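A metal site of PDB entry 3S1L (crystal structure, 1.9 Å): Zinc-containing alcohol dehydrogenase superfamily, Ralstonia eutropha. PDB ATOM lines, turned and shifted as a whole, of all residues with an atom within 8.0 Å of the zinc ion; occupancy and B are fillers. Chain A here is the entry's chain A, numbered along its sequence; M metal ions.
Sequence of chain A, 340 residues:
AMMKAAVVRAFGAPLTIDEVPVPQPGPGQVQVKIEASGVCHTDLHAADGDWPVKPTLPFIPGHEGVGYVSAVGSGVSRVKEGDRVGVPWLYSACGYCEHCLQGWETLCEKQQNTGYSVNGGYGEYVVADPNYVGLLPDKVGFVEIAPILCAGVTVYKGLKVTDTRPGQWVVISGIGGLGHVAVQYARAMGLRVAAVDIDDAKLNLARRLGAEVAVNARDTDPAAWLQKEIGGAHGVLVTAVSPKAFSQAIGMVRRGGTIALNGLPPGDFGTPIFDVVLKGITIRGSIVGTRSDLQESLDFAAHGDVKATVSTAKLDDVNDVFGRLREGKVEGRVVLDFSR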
ATOM      1  N   GLY A  38      -9.323  29.553   1.714  1.00  0.00           N
ATOM      2  CA  GLY A  38      -7.942  29.667   1.294  1.00  0.00           C
ATOM      3  C   GLY A  38      -7.774  30.593   0.100  1.00  0.00           C
ATOM      4  O   GLY A  38      -8.653  30.689  -0.761  1.00  0.00           O
ATOM      5  N   VAL A  39      -6.636  31.267   0.062  1.00  0.00           N
ATOM      6  CA  VAL A  39      -6.289  32.126  -1.067  1.00  0.00           C
ATOM      7  C   VAL A  39      -5.042  31.591  -1.731  1.00  0.00           C
ATOM      8  O   VAL A  39      -4.097  31.176  -1.051  1.00  0.00           O
ATOM      9  CB  VAL A  39      -6.018  33.576  -0.606  1.00  0.00           C
ATOM     10  CG1 VAL A  39      -5.692  34.463  -1.789  1.00  0.00           C
ATOM     11  CG2 VAL A  39      -7.208  34.125   0.162  1.00  0.00           C
ATOM     12  N   CYS A  40      -5.013  31.597  -3.057  1.00  0.00           N
ATOM     13  CA  CYS A  40      -3.804  31.216  -3.781  1.00  0.00           C
ATOM     14  C   CYS A  40      -3.700  31.928  -5.113  1.00  0.00           C
ATOM     15  O   CYS A  40      -4.609  32.668  -5.511  1.00  0.00           O
ATOM     16  CB  CYS A  40      -3.730  29.694  -3.974  1.00  0.00           C
ATOM     17  SG  CYS A  40      -4.586  29.079  -5.421  1.00  0.00           S
ATOM     18  N   HIS A  41      -2.584  31.716  -5.807  1.00  0.00           N
ATOM     19  CA  HIS A  41      -2.302  32.432  -7.050  1.00  0.00           C
ATOM     20  C   HIS A  41      -3.343  32.195  -8.144  1.00  0.00           C
ATOM     21  O   HIS A  41      -3.493  33.028  -9.029  1.00  0.00           O
ATOM     22  CB  HIS A  41      -0.906  32.093  -7.561  1.00  0.00           C
ATOM     23  CG  HIS A  41       0.183  32.809  -6.821  1.00  0.00           C
ATOM     24  ND1 HIS A  41       0.845  32.264  -5.745  1.00  0.00           N
ATOM     25  CD2 HIS A  41       0.715  34.043  -6.986  1.00  0.00           C
ATOM     26  CE1 HIS A  41       1.741  33.118  -5.287  1.00  0.00           C
ATOM     27  NE2 HIS A  41       1.681  34.218  -6.029  1.00  0.00           N
ATOM     28  N   THR A  42      -4.055  31.088  -8.069  1.00  0.00           N
ATOM     29  CA  THR A  42      -5.111  30.808  -9.041  1.00  0.00           C
ATOM     30  C   THR A  42      -6.178  31.901  -8.968  1.00  0.00           C
ATOM     31  O   THR A  42      -6.771  32.282  -9.984  1.00  0.00           O
ATOM     32  CB  THR A  42      -5.739  29.425  -8.804  1.00  0.00           C
ATOM     33  OG1 THR A  42      -4.747  28.417  -9.033  1.00  0.00           O
ATOM     34  CG2 THR A  42      -6.915  29.210  -9.739  1.00  0.00           C
ATOM     35  N   ASP A  43      -6.395  32.412  -7.759  1.00  0.00           N
ATOM     36  CA  ASP A  43      -7.352  33.497  -7.547  1.00  0.00           C
ATOM     37  C   ASP A  43      -6.869  34.781  -8.225  1.00  0.00           C
ATOM     38  O   ASP A  43      -7.672  35.532  -8.768  1.00  0.00           O
ATOM     39  CB  ASP A  43      -7.573  33.722  -6.055  1.00  0.00           C
ATOM     40  CG  ASP A  43      -8.230  32.526  -5.374  1.00  0.00           C
ATOM     41  OD1 ASP A  43      -9.161  31.949  -5.971  1.00  0.00           O
ATOM     42  OD2 ASP A  43      -7.819  32.176  -4.251  1.00  0.00           O
ATOM     43  N   GLY A  62     -12.621  31.965  -5.125  1.00  0.00           N
ATOM     44  CA  GLY A  62     -12.431  31.129  -3.946  1.00  0.00           C
ATOM     45  C   GLY A  62     -12.789  29.666  -4.142  1.00  0.00           C
ATOM     46  O   GLY A  62     -13.965  29.305  -4.138  1.00  0.00           O
ATOM     47  N   HIS A  63     -11.773  28.824  -4.296  1.00  0.00           N
ATOM     48  CA  HIS A  63     -11.980  27.399  -4.480  1.00  0.00           C
ATOM     49  C   HIS A  63     -11.386  26.615  -3.298  1.00  0.00           C
ATOM     50  O   HIS A  63     -11.096  25.431  -3.412  1.00  0.00           O
ATOM     51  CB  HIS A  63     -11.319  26.929  -5.765  1.00  0.00           C
ATOM     52  CG  HIS A  63      -9.893  27.382  -5.889  1.00  0.00           C
ATOM     53  ND1 HIS A  63      -9.547  28.621  -6.378  1.00  0.00           N
ATOM     54  CD2 HIS A  63      -8.739  26.774  -5.550  1.00  0.00           C
ATOM     55  CE1 HIS A  63      -8.237  28.752  -6.339  1.00  0.00           C
ATOM     56  NE2 HIS A  63      -7.716  27.645  -5.853  1.00  0.00           N
ATOM     57  N   GLU A  64     -11.211  27.297  -2.168  1.00  0.00           N
ATOM     58  CA  GLU A  64     -10.657  26.665  -0.979  1.00  0.00           C
ATOM     59  C   GLU A  64     -11.526  26.991   0.230  1.00  0.00           C
ATOM     60  O   GLU A  64     -11.032  27.137   1.340  1.00  0.00           O
ATOM     61  CB  GLU A  64      -9.220  27.139  -0.737  1.00  0.00           C
ATOM     62  CG  GLU A  64      -8.247  26.799  -1.870  1.00  0.00           C
ATOM     63  CD  GLU A  64      -6.828  27.269  -1.612  1.00  0.00           C
ATOM     64  OE1 GLU A  64      -6.406  27.298  -0.437  1.00  0.00           O
ATOM     65  OE2 GLU A  64      -6.133  27.618  -2.579  1.00  0.00           O
ATOM     66  N   TRP A  89     -11.917  23.242  -6.208  1.00  0.00           N
ATOM     67  CA  TRP A  89     -11.890  23.653  -7.603  1.00  0.00           C
ATOM     68  C   TRP A  89     -12.911  22.918  -8.469  1.00  0.00           C
ATOM     69  O   TRP A  89     -13.650  23.542  -9.233  1.00  0.00           O
ATOM     70  CB  TRP A  89     -10.479  23.460  -8.159  1.00  0.00           C
ATOM     71  CG  TRP A  89     -10.324  23.761  -9.606  1.00  0.00           C
ATOM     72  CD1 TRP A  89     -10.110  22.865 -10.621  1.00  0.00           C
ATOM     73  CD2 TRP A  89     -10.343  25.059 -10.222  1.00  0.00           C
ATOM     74  NE1 TRP A  89      -9.994  23.519 -11.819  1.00  0.00           N
ATOM     75  CE2 TRP A  89     -10.137  24.869 -11.604  1.00  0.00           C
ATOM     76  CE3 TRP A  89     -10.514  26.358  -9.746  1.00  0.00           C
ATOM     77  CZ2 TRP A  89     -10.105  25.924 -12.509  1.00  0.00           C
ATOM     78  CZ3 TRP A  89     -10.472  27.410 -10.642  1.00  0.00           C
ATOM     79  CH2 TRP A  89     -10.274  27.181 -12.005  1.00  0.00           C
ATOM     80  N   TYR A 122     -15.189  33.189  -1.393  1.00  0.00           N
ATOM     81  CA  TYR A 122     -14.910  34.518  -0.835  1.00  0.00           C
ATOM     82  C   TYR A 122     -16.213  35.186  -0.388  1.00  0.00           C
ATOM     83  O   TYR A 122     -16.471  36.342  -0.710  1.00  0.00           O
ATOM     84  CB  TYR A 122     -14.239  35.427  -1.858  1.00  0.00           C
ATOM     85  CG  TYR A 122     -12.779  35.154  -2.143  1.00  0.00           C
ATOM     86  CD1 TYR A 122     -12.021  36.075  -2.853  1.00  0.00           C
ATOM     87  CD2 TYR A 122     -12.158  33.982  -1.723  1.00  0.00           C
ATOM     88  CE1 TYR A 122     -10.691  35.848  -3.124  1.00  0.00           C
ATOM     89  CE2 TYR A 122     -10.822  33.744  -2.002  1.00  0.00           C
ATOM     90  CZ  TYR A 122     -10.087  34.688  -2.707  1.00  0.00           C
ATOM     91  OH  TYR A 122      -8.765  34.495  -3.003  1.00  0.00           O
ATOM     92  N   ALA A 146      -8.056  24.141   5.026  1.00  0.00           N
ATOM     93  CA  ALA A 146      -8.433  24.795   3.762  1.00  0.00           C
ATOM     94  C   ALA A 146      -7.471  24.582   2.587  1.00  0.00           C
ATOM     95  O   ALA A 146      -7.901  24.205   1.490  1.00  0.00           O
ATOM     96  CB  ALA A 146      -8.694  26.293   3.988  1.00  0.00           C
ATOM     97  N   PRO A 147      -6.158  24.832   2.783  1.00  0.00           N
ATOM     98  CA  PRO A 147      -5.220  24.697   1.655  1.00  0.00           C
ATOM     99  C   PRO A 147      -5.092  23.265   1.136  1.00  0.00           C
ATOM    100  O   PRO A 147      -4.629  23.068   0.010  1.00  0.00           O
ATOM    101  CB  PRO A 147      -3.886  25.143   2.260  1.00  0.00           C
ATOM    102  CG  PRO A 147      -4.242  25.924   3.485  1.00  0.00           C
ATOM    103  CD  PRO A 147      -5.480  25.282   4.014  1.00  0.00           C
ATOM    104  N   LEU A 149      -7.433  21.461   0.227  1.00  0.00           N
ATOM    105  CA  LEU A 149      -8.381  21.380  -0.885  1.00  0.00           C
ATOM    106  C   LEU A 149      -7.742  21.729  -2.219  1.00  0.00           C
ATOM    107  O   LEU A 149      -8.292  21.418  -3.279  1.00  0.00           O
ATOM    108  CB  LEU A 149      -9.567  22.327  -0.671  1.00  0.00           C
ATOM    109  CG  LEU A 149     -10.467  22.091   0.537  1.00  0.00           C
ATOM    110  CD1 LEU A 149     -11.584  23.124   0.557  1.00  0.00           C
ATOM    111  CD2 LEU A 149     -11.049  20.698   0.505  1.00  0.00           C
ATOM    112  N   CYS A 150      -6.601  22.408  -2.170  1.00  0.00           N
ATOM    113  CA  CYS A 150      -5.962  22.920  -3.376  1.00  0.00           C
ATOM    114  C   CYS A 150      -4.496  22.511  -3.447  1.00  0.00           C
ATOM    115  O   CYS A 150      -4.126  21.635  -4.234  1.00  0.00           O
ATOM    116  CB  CYS A 150      -6.088  24.441  -3.429  1.00  0.00           C
ATOM    117  SG  CYS A 150      -5.242  25.174  -4.815  1.00  0.00           S
ATOM    118  N   ALA A 151      -3.664  23.136  -2.621  1.00  0.00           N
ATOM    119  CA  ALA A 151      -2.253  22.756  -2.528  1.00  0.00           C
ATOM    120  C   ALA A 151      -2.110  21.278  -2.209  1.00  0.00           C
ATOM    121  O   ALA A 151      -1.339  20.561  -2.862  1.00  0.00           O
ATOM    122  CB  ALA A 151      -1.552  23.590  -1.461  1.00  0.00           C
ATOM    123  N   THR A 154      -3.316  18.862  -4.990  1.00  0.00           N
ATOM    124  CA  THR A 154      -2.480  19.070  -6.164  1.00  0.00           C
ATOM    125  C   THR A 154      -1.143  18.338  -6.068  1.00  0.00           C
ATOM    126  O   THR A 154      -0.775  17.619  -6.979  1.00  0.00           O
ATOM    127  CB  THR A 154      -2.246  20.569  -6.471  1.00  0.00           C
ATOM    128  OG1 THR A 154      -3.462  21.133  -6.945  1.00  0.00           O
ATOM    129  CG2 THR A 154      -1.166  20.737  -7.537  1.00  0.00           C
ATOM    130  N   LEU A 178       3.241  25.384  -2.351  1.00  0.00           N
ATOM    131  CA  LEU A 178       2.967  23.987  -2.702  1.00  0.00           C
ATOM    132  C   LEU A 178       4.046  23.044  -2.190  1.00  0.00           C
ATOM    133  O   LEU A 178       3.762  21.980  -1.657  1.00  0.00           O
ATOM    134  CB  LEU A 178       2.850  23.824  -4.228  1.00  0.00           C
ATOM    135  CG  LEU A 178       1.608  24.394  -4.922  1.00  0.00           C
ATOM    136  CD1 LEU A 178       1.721  24.222  -6.429  1.00  0.00           C
ATOM    137  CD2 LEU A 178       0.362  23.703  -4.415  1.00  0.00           C
ATOM    138  N   VAL A 288      -4.509  19.752  -9.493  1.00  0.00           N
ATOM    139  CA  VAL A 288      -5.611  19.292  -8.637  1.00  0.00           C
ATOM    140  C   VAL A 288      -5.788  17.774  -8.643  1.00  0.00           C
ATOM    141  O   VAL A 288      -4.814  17.024  -8.728  1.00  0.00           O
ATOM    142  CB  VAL A 288      -6.951  20.054  -8.901  1.00  0.00           C
ATOM    143  CG1 VAL A 288      -6.845  21.480  -8.377  1.00  0.00           C
ATOM    144  CG2 VAL A 288      -7.317  20.053 -10.386  1.00  0.00           C
ATOM    145  N   ARG A 333       0.869  29.569   3.148  1.00  0.00           N
ATOM    146  CA  ARG A 333      -0.411  29.864   2.515  1.00  0.00           C
ATOM    147  C   ARG A 333      -1.186  30.865   3.352  1.00  0.00           C
ATOM    148  O   ARG A 333      -1.046  30.912   4.570  1.00  0.00           O
ATOM    149  CB  ARG A 333      -1.249  28.592   2.353  1.00  0.00           C
ATOM    150  CG  ARG A 333      -0.563  27.494   1.542  1.00  0.00           C
ATOM    151  CD  ARG A 333      -0.613  27.799   0.053  1.00  0.00           C
ATOM    152  NE  ARG A 333      -1.940  27.574  -0.507  1.00  0.00           N
ATOM    153  CZ  ARG A 333      -2.182  27.231  -1.764  1.00  0.00           C
ATOM    154  NH1 ARG A 333      -1.177  27.057  -2.621  1.00  0.00           N
ATOM    155  NH2 ARG A 333      -3.438  27.048  -2.178  1.00  0.00           N
HETATM  156 ZN    ZN M   1      -6.023  27.453  -4.609  1.00  0.00          ZN
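The side-chain carboxylate (OE1) of Glu 64 lies within salt-bridge range of the guanidinium group (NH2) of Arg 333, at 3.5 Å.
O of Glu 64 lies within hydrogen-bond range of N of Gly 38 (3.0 Å).
ND1 of His 63 sits close to OD1 of Asp 43, at 3.4 Å.
The side-chain sulfur of Cys 40 sits close to the backbone NH of Thr 42 (3.4 Å).
N of Cys 40 lies within hydrogen-bond range of OD2 of Asp 43.
The side-chain sulfur of Cys 150 lies close to the guanidinium group of Arg 333 (3.7 Å).
The backbone carbonyl oxygen (O) of Cys 150 lies within hydrogen-bond range of the side-chain hydroxyl (OG1) of Thr 154, 2.8 Å away.
OE2 of Glu 64 is bound to the zinc ion (2.0 Å).
A ring nitrogen (NE2) of His 63 is bound to the zinc ion (2.1 Å).
The zinc ion is bound by the side-chain sulfur (SG) of Cys 40, 2.3 Å away.
The zinc ion is bound by SG of Cys 150.
Merely in contact with the zinc ion: Arg 333 (3.6 Å).
Of the 20 residues printed, 5 come within 4 Å of the zinc ion.
Along chain A the residues within 4 Å of the zinc ion span positions 40 to 333.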
